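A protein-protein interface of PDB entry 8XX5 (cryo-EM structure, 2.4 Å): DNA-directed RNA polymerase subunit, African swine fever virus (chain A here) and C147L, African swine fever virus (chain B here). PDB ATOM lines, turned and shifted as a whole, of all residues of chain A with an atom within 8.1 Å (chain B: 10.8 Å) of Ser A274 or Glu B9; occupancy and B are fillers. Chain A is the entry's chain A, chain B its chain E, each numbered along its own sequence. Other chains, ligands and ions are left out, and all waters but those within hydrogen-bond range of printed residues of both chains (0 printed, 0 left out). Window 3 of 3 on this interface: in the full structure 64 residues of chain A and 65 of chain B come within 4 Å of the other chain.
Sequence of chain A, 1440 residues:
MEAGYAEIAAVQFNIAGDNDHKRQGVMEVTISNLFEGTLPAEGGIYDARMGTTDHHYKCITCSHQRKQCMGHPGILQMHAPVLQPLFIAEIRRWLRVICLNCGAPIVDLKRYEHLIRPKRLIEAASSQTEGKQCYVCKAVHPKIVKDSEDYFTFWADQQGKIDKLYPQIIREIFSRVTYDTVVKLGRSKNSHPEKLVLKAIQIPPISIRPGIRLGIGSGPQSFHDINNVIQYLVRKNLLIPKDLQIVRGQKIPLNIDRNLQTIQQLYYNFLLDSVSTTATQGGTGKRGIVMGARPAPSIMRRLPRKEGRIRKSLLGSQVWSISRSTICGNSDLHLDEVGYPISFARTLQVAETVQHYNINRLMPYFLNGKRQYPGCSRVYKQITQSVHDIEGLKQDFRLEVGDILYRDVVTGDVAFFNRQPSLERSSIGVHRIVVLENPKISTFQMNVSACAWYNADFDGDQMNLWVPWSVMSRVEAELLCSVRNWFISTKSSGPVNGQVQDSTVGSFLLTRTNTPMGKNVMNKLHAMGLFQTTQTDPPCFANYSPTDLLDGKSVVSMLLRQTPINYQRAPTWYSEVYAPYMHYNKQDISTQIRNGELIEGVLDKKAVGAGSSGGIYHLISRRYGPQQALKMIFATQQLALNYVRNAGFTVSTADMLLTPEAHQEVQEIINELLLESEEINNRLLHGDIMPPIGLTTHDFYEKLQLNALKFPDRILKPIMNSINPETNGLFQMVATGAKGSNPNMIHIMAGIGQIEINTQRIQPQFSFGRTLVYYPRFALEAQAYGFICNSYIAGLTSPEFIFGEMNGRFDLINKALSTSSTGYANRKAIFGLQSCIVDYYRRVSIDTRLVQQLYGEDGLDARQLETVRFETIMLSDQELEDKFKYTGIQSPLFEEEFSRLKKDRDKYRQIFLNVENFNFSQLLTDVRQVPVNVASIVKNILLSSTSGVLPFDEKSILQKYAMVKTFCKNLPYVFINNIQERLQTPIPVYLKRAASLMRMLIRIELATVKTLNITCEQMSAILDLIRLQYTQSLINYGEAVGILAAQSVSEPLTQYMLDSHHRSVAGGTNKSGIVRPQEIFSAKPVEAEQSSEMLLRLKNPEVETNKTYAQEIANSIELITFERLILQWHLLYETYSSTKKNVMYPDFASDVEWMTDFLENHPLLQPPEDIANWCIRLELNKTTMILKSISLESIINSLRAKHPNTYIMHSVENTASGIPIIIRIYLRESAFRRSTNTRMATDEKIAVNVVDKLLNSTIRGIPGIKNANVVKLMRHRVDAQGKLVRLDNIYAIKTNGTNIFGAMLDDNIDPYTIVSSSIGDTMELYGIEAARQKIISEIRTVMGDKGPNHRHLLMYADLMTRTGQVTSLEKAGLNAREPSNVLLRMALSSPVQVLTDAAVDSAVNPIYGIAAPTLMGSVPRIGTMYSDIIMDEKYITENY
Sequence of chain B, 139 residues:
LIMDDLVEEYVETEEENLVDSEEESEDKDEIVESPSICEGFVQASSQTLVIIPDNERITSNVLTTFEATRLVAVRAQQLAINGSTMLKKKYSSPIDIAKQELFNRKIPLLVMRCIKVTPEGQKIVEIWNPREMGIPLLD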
ATOM      1  N   TYR A 151      21.712  -8.546 -27.747  1.00  0.00           N
ATOM      2  CA  TYR A 151      21.867  -7.524 -26.722  1.00  0.00           C
ATOM      3  C   TYR A 151      23.139  -6.701 -26.875  1.00  0.00           C
ATOM      4  O   TYR A 151      23.425  -5.867 -26.011  1.00  0.00           O
ATOM      5  CB  TYR A 151      21.841  -8.166 -25.336  1.00  0.00           C
ATOM      6  CG  TYR A 151      20.630  -9.026 -25.065  1.00  0.00           C
ATOM      7  CD1 TYR A 151      19.371  -8.462 -24.929  1.00  0.00           C
ATOM      8  CD2 TYR A 151      20.749 -10.402 -24.936  1.00  0.00           C
ATOM      9  CE1 TYR A 151      18.264  -9.244 -24.676  1.00  0.00           C
ATOM     10  CE2 TYR A 151      19.647 -11.192 -24.682  1.00  0.00           C
ATOM     11  CZ  TYR A 151      18.407 -10.608 -24.553  1.00  0.00           C
ATOM     12  OH  TYR A 151      17.306 -11.392 -24.301  1.00  0.00           O
ATOM     13  N   TYR A 268      28.563 -12.845 -23.598  1.00  0.00           N
ATOM     14  CA  TYR A 268      27.369 -12.265 -22.997  1.00  0.00           C
ATOM     15  C   TYR A 268      26.593 -13.300 -22.195  1.00  0.00           C
ATOM     16  O   TYR A 268      26.010 -12.975 -21.161  1.00  0.00           O
ATOM     17  CB  TYR A 268      26.479 -11.642 -24.072  1.00  0.00           C
ATOM     18  CG  TYR A 268      25.408 -10.740 -23.504  1.00  0.00           C
ATOM     19  CD1 TYR A 268      24.186 -11.253 -23.092  1.00  0.00           C
ATOM     20  CD2 TYR A 268      25.625  -9.378 -23.369  1.00  0.00           C
ATOM     21  CE1 TYR A 268      23.212 -10.432 -22.564  1.00  0.00           C
ATOM     22  CE2 TYR A 268      24.656  -8.550 -22.844  1.00  0.00           C
ATOM     23  CZ  TYR A 268      23.451  -9.083 -22.442  1.00  0.00           C
ATOM     24  OH  TYR A 268      22.482  -8.259 -21.921  1.00  0.00           O
ATOM     25  N   ASN A 269      26.549 -14.545 -22.665  1.00  0.00           N
ATOM     26  CA  ASN A 269      25.882 -15.593 -21.903  1.00  0.00           C
ATOM     27  C   ASN A 269      26.714 -16.041 -20.711  1.00  0.00           C
ATOM     28  O   ASN A 269      26.158 -16.478 -19.700  1.00  0.00           O
ATOM     29  CB  ASN A 269      25.569 -16.788 -22.802  1.00  0.00           C
ATOM     30  CG  ASN A 269      24.659 -16.426 -23.952  1.00  0.00           C
ATOM     31  OD1 ASN A 269      24.060 -15.352 -23.970  1.00  0.00           O
ATOM     32  ND2 ASN A 269      24.546 -17.325 -24.921  1.00  0.00           N
ATOM     33  N   LEU A 271      28.443 -13.994 -18.884  1.00  0.00           N
ATOM     34  CA  LEU A 271      28.287 -12.990 -17.838  1.00  0.00           C
ATOM     35  C   LEU A 271      26.833 -12.770 -17.418  1.00  0.00           C
ATOM     36  O   LEU A 271      26.537 -12.735 -16.221  1.00  0.00           O
ATOM     37  CB  LEU A 271      28.916 -11.667 -18.284  1.00  0.00           C
ATOM     38  CG  LEU A 271      30.447 -11.633 -18.269  1.00  0.00           C
ATOM     39  CD1 LEU A 271      30.956 -10.205 -18.292  1.00  0.00           C
ATOM     40  CD2 LEU A 271      30.992 -12.371 -17.059  1.00  0.00           C
ATOM     41  N   LEU A 272      25.916 -12.637 -18.373  1.00  0.00           N
ATOM     42  CA  LEU A 272      24.569 -12.129 -18.128  1.00  0.00           C
ATOM     43  C   LEU A 272      23.505 -12.997 -18.789  1.00  0.00           C
ATOM     44  O   LEU A 272      22.557 -12.487 -19.390  1.00  0.00           O
ATOM     45  CB  LEU A 272      24.437 -10.693 -18.623  1.00  0.00           C
ATOM     46  CG  LEU A 272      24.918  -9.560 -17.722  1.00  0.00           C
ATOM     47  CD1 LEU A 272      24.844  -8.244 -18.472  1.00  0.00           C
ATOM     48  CD2 LEU A 272      24.089  -9.501 -16.458  1.00  0.00           C
ATOM     49  N   ASP A 273      23.628 -14.317 -18.690  1.00  0.00           N
ATOM     50  CA  ASP A 273      22.594 -15.205 -19.207  1.00  0.00           C
ATOM     51  C   ASP A 273      21.460 -15.326 -18.198  1.00  0.00           C
ATOM     52  O   ASP A 273      21.701 -15.474 -16.997  1.00  0.00           O
ATOM     53  CB  ASP A 273      23.168 -16.586 -19.514  1.00  0.00           C
ATOM     54  CG  ASP A 273      22.275 -17.400 -20.427  1.00  0.00           C
ATOM     55  OD1 ASP A 273      22.052 -16.975 -21.579  1.00  0.00           O
ATOM     56  OD2 ASP A 273      21.800 -18.471 -19.994  1.00  0.00           O
ATOM     57  N   SER A 274      20.225 -15.260 -18.695  1.00  0.00           N
ATOM     58  CA  SER A 274      19.010 -15.405 -17.893  1.00  0.00           C
ATOM     59  C   SER A 274      18.843 -14.289 -16.868  1.00  0.00           C
ATOM     60  O   SER A 274      18.135 -14.463 -15.871  1.00  0.00           O
ATOM     61  CB  SER A 274      18.960 -16.772 -17.198  1.00  0.00           C
ATOM     62  OG  SER A 274      18.202 -17.701 -17.952  1.00  0.00           O
ATOM     63  N   VAL A 275      19.482 -13.142 -17.086  1.00  0.00           N
ATOM     64  CA  VAL A 275      19.270 -11.950 -16.274  1.00  0.00           C
ATOM     65  C   VAL A 275      19.034 -10.783 -17.224  1.00  0.00           C
ATOM     66  O   VAL A 275      19.800 -10.590 -18.175  1.00  0.00           O
ATOM     67  CB  VAL A 275      20.457 -11.672 -15.327  1.00  0.00           C
ATOM     68  CG1 VAL A 275      21.697 -12.426 -15.776  1.00  0.00           C
ATOM     69  CG2 VAL A 275      20.731 -10.176 -15.206  1.00  0.00           C
ATOM     70  N   SER A 276      17.967 -10.021 -16.982  1.00  0.00           N
ATOM     71  CA  SER A 276      17.560  -8.995 -17.937  1.00  0.00           C
ATOM     72  C   SER A 276      18.132  -7.619 -17.603  1.00  0.00           C
ATOM     73  O   SER A 276      18.944  -7.088 -18.365  1.00  0.00           O
ATOM     74  CB  SER A 276      16.031  -8.928 -18.014  1.00  0.00           C
ATOM     75  OG  SER A 276      15.501 -10.102 -18.601  1.00  0.00           O
ATOM     76  N   THR A 277      17.727  -7.042 -16.466  1.00  0.00           N
ATOM     77  CA  THR A 277      18.133  -5.701 -16.039  1.00  0.00           C
ATOM     78  C   THR A 277      17.550  -4.631 -16.965  1.00  0.00           C
ATOM     79  O   THR A 277      17.447  -4.839 -18.178  1.00  0.00           O
ATOM     80  CB  THR A 277      19.667  -5.605 -15.952  1.00  0.00           C
ATOM     81  OG1 THR A 277      20.120  -6.243 -14.750  1.00  0.00           O
ATOM     82  CG2 THR A 277      20.148  -4.163 -15.964  1.00  0.00           C
ATOM     83  N   THR A 280      19.340  -3.238 -20.228  1.00  0.00           N
ATOM     84  CA  THR A 280      19.564  -4.166 -21.331  1.00  0.00           C
ATOM     85  C   THR A 280      18.926  -3.596 -22.592  1.00  0.00           C
ATOM     86  O   THR A 280      17.717  -3.344 -22.628  1.00  0.00           O
ATOM     87  CB  THR A 280      18.994  -5.541 -21.003  1.00  0.00           C
ATOM     88  OG1 THR A 280      19.921  -6.252 -20.175  1.00  0.00           O
ATOM     89  CG2 THR A 280      18.749  -6.338 -22.266  1.00  0.00           C
ATOM     90  N   ALA A 296      23.630 -23.645 -17.927  1.00  0.00           N
ATOM     91  CA  ALA A 296      24.840 -22.959 -17.490  1.00  0.00           C
ATOM     92  C   ALA A 296      24.517 -21.576 -16.933  1.00  0.00           C
ATOM     93  O   ALA A 296      24.541 -20.590 -17.671  1.00  0.00           O
ATOM     94  CB  ALA A 296      25.828 -22.849 -18.638  1.00  0.00           C
ATOM     95  N   PRO A 297      24.196 -21.509 -15.640  1.00  0.00           N
ATOM     96  CA  PRO A 297      23.930 -20.205 -15.013  1.00  0.00           C
ATOM     97  C   PRO A 297      25.129 -19.280 -15.157  1.00  0.00           C
ATOM     98  O   PRO A 297      26.277 -19.698 -14.990  1.00  0.00           O
ATOM     99  CB  PRO A 297      23.661 -20.549 -13.542  1.00  0.00           C
ATOM    100  CG  PRO A 297      23.538 -22.028 -13.460  1.00  0.00           C
ATOM    101  CD  PRO A 297      23.856 -22.650 -14.775  1.00  0.00           C
ATOM    102  N   SER A 298      24.853 -18.017 -15.464  1.00  0.00           N
ATOM    103  CA  SER A 298      25.916 -17.056 -15.693  1.00  0.00           C
ATOM    104  C   SER A 298      26.517 -16.589 -14.368  1.00  0.00           C
ATOM    105  O   SER A 298      26.090 -16.982 -13.281  1.00  0.00           O
ATOM    106  CB  SER A 298      25.391 -15.863 -16.485  1.00  0.00           C
ATOM    107  OG  SER A 298      24.075 -15.532 -16.087  1.00  0.00           O
ATOM    108  N   MET A 300      26.493 -13.414 -13.243  1.00  0.00           N
ATOM    109  CA  MET A 300      25.572 -12.494 -12.587  1.00  0.00           C
ATOM    110  C   MET A 300      24.274 -13.166 -12.167  1.00  0.00           C
ATOM    111  O   MET A 300      23.538 -12.603 -11.352  1.00  0.00           O
ATOM    112  CB  MET A 300      25.274 -11.307 -13.501  1.00  0.00           C
ATOM    113  CG  MET A 300      26.494 -10.474 -13.867  1.00  0.00           C
ATOM    114  SD  MET A 300      26.979  -9.295 -12.590  1.00  0.00           S
ATOM    115  CE  MET A 300      28.160 -10.256 -11.646  1.00  0.00           C
ATOM    116  N   ARG A 301      23.968 -14.346 -12.706  1.00  0.00           N
ATOM    117  CA  ARG A 301      22.794 -15.083 -12.263  1.00  0.00           C
ATOM    118  C   ARG A 301      23.000 -15.735 -10.902  1.00  0.00           C
ATOM    119  O   ARG A 301      22.018 -16.067 -10.231  1.00  0.00           O
ATOM    120  CB  ARG A 301      22.420 -16.144 -13.301  1.00  0.00           C
ATOM    121  CG  ARG A 301      21.030 -16.729 -13.129  1.00  0.00           C
ATOM    122  CD  ARG A 301      19.976 -15.638 -13.096  1.00  0.00           C
ATOM    123  NE  ARG A 301      18.641 -16.173 -12.856  1.00  0.00           N
ATOM    124  CZ  ARG A 301      18.165 -16.493 -11.661  1.00  0.00           C
ATOM    125  NH1 ARG A 301      18.890 -16.347 -10.566  1.00  0.00           N
ATOM    126  NH2 ARG A 301      16.927 -16.969 -11.563  1.00  0.00           N
ATOM    127  N   PRO A 304      21.553 -12.863  -7.460  1.00  0.00           N
ATOM    128  CA  PRO A 304      20.288 -12.364  -6.915  1.00  0.00           C
ATOM    129  C   PRO A 304      19.413 -13.469  -6.335  1.00  0.00           C
ATOM    130  O   PRO A 304      19.689 -14.661  -6.462  1.00  0.00           O
ATOM    131  CB  PRO A 304      19.626 -11.725  -8.132  1.00  0.00           C
ATOM    132  CG  PRO A 304      20.059 -12.586  -9.245  1.00  0.00           C
ATOM    133  CD  PRO A 304      21.467 -13.015  -8.925  1.00  0.00           C
ATOM    134  N   ARG A 305      18.340 -13.022  -5.675  1.00  0.00           N
ATOM    135  CA  ARG A 305      17.273 -13.859  -5.127  1.00  0.00           C
ATOM    136  C   ARG A 305      17.723 -14.647  -3.903  1.00  0.00           C
ATOM    137  O   ARG A 305      18.895 -14.600  -3.516  1.00  0.00           O
ATOM    138  CB  ARG A 305      16.718 -14.798  -6.200  1.00  0.00           C
ATOM    139  CG  ARG A 305      16.089 -14.067  -7.377  1.00  0.00           C
ATOM    140  CD  ARG A 305      15.233 -14.993  -8.214  1.00  0.00           C
ATOM    141  NE  ARG A 305      13.910 -15.174  -7.631  1.00  0.00           N
ATOM    142  CZ  ARG A 305      13.267 -16.332  -7.577  1.00  0.00           C
ATOM    143  NH1 ARG A 305      13.794 -17.439  -8.076  1.00  0.00           N
ATOM    144  NH2 ARG A 305      12.065 -16.381  -7.011  1.00  0.00           N
ATOM    145  N   ASP B   5      14.818 -29.046 -15.809  1.00  0.00           N
ATOM    146  CA  ASP B   5      15.590 -28.128 -14.980  1.00  0.00           C
ATOM    147  C   ASP B   5      15.726 -26.755 -15.628  1.00  0.00           C
ATOM    148  O   ASP B   5      16.795 -26.407 -16.139  1.00  0.00           O
ATOM    149  CB  ASP B   5      16.975 -28.711 -14.689  1.00  0.00           C
ATOM    150  CG  ASP B   5      16.935 -30.202 -14.425  1.00  0.00           C
ATOM    151  OD1 ASP B   5      16.679 -30.595 -13.267  1.00  0.00           O
ATOM    152  OD2 ASP B   5      17.163 -30.982 -15.373  1.00  0.00           O
ATOM    153  N   LEU B   6      14.653 -25.969 -15.612  1.00  0.00           N
ATOM    154  CA  LEU B   6      14.724 -24.607 -16.116  1.00  0.00           C
ATOM    155  C   LEU B   6      15.362 -23.687 -15.081  1.00  0.00           C
ATOM    156  O   LEU B   6      15.435 -24.001 -13.889  1.00  0.00           O
ATOM    157  CB  LEU B   6      13.336 -24.094 -16.497  1.00  0.00           C
ATOM    158  CG  LEU B   6      12.829 -24.553 -17.867  1.00  0.00           C
ATOM    159  CD1 LEU B   6      11.816 -23.569 -18.424  1.00  0.00           C
ATOM    160  CD2 LEU B   6      13.987 -24.741 -18.834  1.00  0.00           C
ATOM    161  N   VAL B   7      15.829 -22.532 -15.552  1.00  0.00           N
ATOM    162  CA  VAL B   7      16.602 -21.623 -14.718  1.00  0.00           C
ATOM    163  C   VAL B   7      15.818 -20.393 -14.276  1.00  0.00           C
ATOM    164  O   VAL B   7      16.345 -19.609 -13.471  1.00  0.00           O
ATOM    165  CB  VAL B   7      17.907 -21.194 -15.420  1.00  0.00           C
ATOM    166  CG1 VAL B   7      19.107 -21.524 -14.547  1.00  0.00           C
ATOM    167  CG2 VAL B   7      18.027 -21.867 -16.777  1.00  0.00           C
ATOM    168  N   GLU B   8      14.589 -20.197 -14.761  1.00  0.00           N
ATOM    169  CA  GLU B   8      13.750 -19.093 -14.301  1.00  0.00           C
ATOM    170  C   GLU B   8      14.399 -17.732 -14.529  1.00  0.00           C
ATOM    171  O   GLU B   8      14.861 -17.105 -13.571  1.00  0.00           O
ATOM    172  CB  GLU B   8      13.396 -19.258 -12.822  1.00  0.00           C
ATOM    173  CG  GLU B   8      11.994 -18.783 -12.473  1.00  0.00           C
ATOM    174  CD  GLU B   8      11.539 -19.260 -11.110  1.00  0.00           C
ATOM    175  OE1 GLU B   8      10.318 -19.436 -10.917  1.00  0.00           O
ATOM    176  OE2 GLU B   8      12.403 -19.452 -10.229  1.00  0.00           O
ATOM    177  N   GLU B   9      14.493 -17.312 -15.793  1.00  0.00           N
ATOM    178  CA  GLU B   9      15.038 -16.007 -16.165  1.00  0.00           C
ATOM    179  C   GLU B   9      14.676 -14.927 -15.152  1.00  0.00           C
ATOM    180  O   GLU B   9      13.526 -14.817 -14.718  1.00  0.00           O
ATOM    181  CB  GLU B   9      14.525 -15.598 -17.546  1.00  0.00           C
ATOM    182  CG  GLU B   9      15.491 -14.746 -18.347  1.00  0.00           C
ATOM    183  CD  GLU B   9      15.153 -13.267 -18.310  1.00  0.00           C
ATOM    184  OE1 GLU B   9      16.028 -12.448 -18.661  1.00  0.00           O
ATOM    185  OE2 GLU B   9      14.012 -12.924 -17.935  1.00  0.00           O
ATOM    186  N   TYR B  10      15.672 -14.128 -14.780  1.00  0.00           N
ATOM    187  CA  TYR B  10      15.564 -13.179 -13.678  1.00  0.00           C
ATOM    188  C   TYR B  10      15.585 -11.758 -14.229  1.00  0.00           C
ATOM    189  O   TYR B  10      16.422 -11.431 -15.077  1.00  0.00           O
ATOM    190  CB  TYR B  10      16.698 -13.406 -12.680  1.00  0.00           C
ATOM    191  CG  TYR B  10      17.025 -12.218 -11.813  1.00  0.00           C
ATOM    192  CD1 TYR B  10      16.296 -11.956 -10.663  1.00  0.00           C
ATOM    193  CD2 TYR B  10      18.074 -11.371 -12.131  1.00  0.00           C
ATOM    194  CE1 TYR B  10      16.592 -10.877  -9.865  1.00  0.00           C
ATOM    195  CE2 TYR B  10      18.377 -10.293 -11.341  1.00  0.00           C
ATOM    196  CZ  TYR B  10      17.631 -10.046 -10.209  1.00  0.00           C
ATOM    197  OH  TYR B  10      17.931  -8.968  -9.409  1.00  0.00           O
ATOM    198  N   VAL B  11      14.666 -10.920 -13.754  1.00  0.00           N
ATOM    199  CA  VAL B  11      14.458  -9.585 -14.302  1.00  0.00           C
ATOM    200  C   VAL B  11      14.531  -8.554 -13.185  1.00  0.00           C
ATOM    201  O   VAL B  11      13.937  -8.736 -12.117  1.00  0.00           O
ATOM    202  CB  VAL B  11      13.107  -9.477 -15.040  1.00  0.00           C
ATOM    203  CG1 VAL B  11      13.059  -8.212 -15.878  1.00  0.00           C
ATOM    204  CG2 VAL B  11      12.866 -10.701 -15.905  1.00  0.00           C
ATOM    205  N   GLU B  12      15.261  -7.472 -13.439  1.00  0.00           N
ATOM    206  CA  GLU B  12      15.251  -6.284 -12.597  1.00  0.00           C
ATOM    207  C   GLU B  12      14.534  -5.174 -13.351  1.00  0.00           C
ATOM    208  O   GLU B  12      14.830  -4.932 -14.526  1.00  0.00           O
ATOM    209  CB  GLU B  12      16.672  -5.851 -12.228  1.00  0.00           C
ATOM    210  CG  GLU B  12      17.657  -6.999 -12.112  1.00  0.00           C
ATOM    211  CD  GLU B  12      18.822  -6.682 -11.196  1.00  0.00           C
ATOM    212  OE1 GLU B  12      19.065  -5.492 -10.935  1.00  0.00           O
ATOM    213  OE2 GLU B  12      19.495  -7.620 -10.726  1.00  0.00           O
ATOM    214  N   THR B  13      13.590  -4.514 -12.688  1.00  0.00           N
ATOM    215  CA  THR B  13      12.723  -3.554 -13.363  1.00  0.00           C
ATOM    216  C   THR B  13      12.790  -2.148 -12.790  1.00  0.00           C
ATOM    217  O   THR B  13      12.667  -1.180 -13.543  1.00  0.00           O
ATOM    218  CB  THR B  13      11.268  -4.043 -13.335  1.00  0.00           C
ATOM    219  OG1 THR B  13      10.795  -4.074 -11.983  1.00  0.00           O
ATOM    220  CG2 THR B  13      11.168  -5.431 -13.941  1.00  0.00           C
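The guanidinium group (NH2) of Arg A301 is in hydrogen-bond range of the backbone carbonyl oxygen (O) of Val B7 (3.3 Å). O of Ser A274 sits at hydrogen-bond distance from N of Tyr B10 (2.7 Å). The guanidinium group (NH2) of Arg A301 is in hydrogen-bond range of the backbone carbonyl oxygen (O) of Glu B8 (2.9 Å). OG of Ser A276 sits at hydrogen-bond distance from OE1 of Glu B9 (2.4 Å). The backbone NH of Ser A276 lies within hydrogen-bond range of the backbone carbonyl oxygen of Tyr B10 (2.8 Å). The guanidinium group (NH1) of Arg A305 is in salt-bridge range of the side-chain carboxylate (OE2) of Glu B8, 3.3 Å away.
The side-chain hydroxyl (OG1) of Thr A280 lies close to the backbone carbonyl oxygen (O) of Thr A277 (3.5 Å). The side-chain hydroxyl of Tyr B10 is in hydrogen-bond range of the side-chain carboxylate of Glu B12 (2.4 Å).
Among the printed residues, merely in contact across the chains: Ser A274 with Glu B9, Val A275 with Glu B9, Val A275 with Tyr B10, Ser A276 with Val B11, Thr A277 with Glu B12, Arg A301 with Tyr B10, Pro A304 with Tyr B10 and Arg A305 with Tyr B10.
Ser A274 touches two residues of chain B. Of the printed residues of chain B, Ser A276 touches Glu B9 (2.4 Å), Tyr B10 (2.8 Å) and Val B11 (3.7 Å). Ala A296 touches none of the printed residues of chain B. Of the printed residues of chain B, Arg A301 touches Val B7, Glu B8 and Tyr B10. Of the printed residues of chain A, Glu B8 touches Arg A301 and Arg A305. The nearest residue of chain A that does not touch Glu B9 is Arg A301 (4.7 Å). The nearest printed residue of chain B that does not touch Arg A305 is Val B7 (6.4 Å).
Printed residues of chain A that touch a printed residue of chain B: Ser A274, Val A275, Ser A276, Thr A277, Arg A301, Pro A304 and Arg A305. Hydrophobic or aromatic side chains of chain A within 4 Å of the printed part of chain B: Val A275 and Pro A304. Hydrophobic or aromatic side chains of chain B that line the printed part of chain A: Tyr B10 and Val B11. Among the printed residues, 14 pairs touch across the chains. Among the printed residues, Asp or Glu carboxylates within 4 Å of a Lys or Arg side-chain nitrogen of the other chain: Arg A305 with Glu B8.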
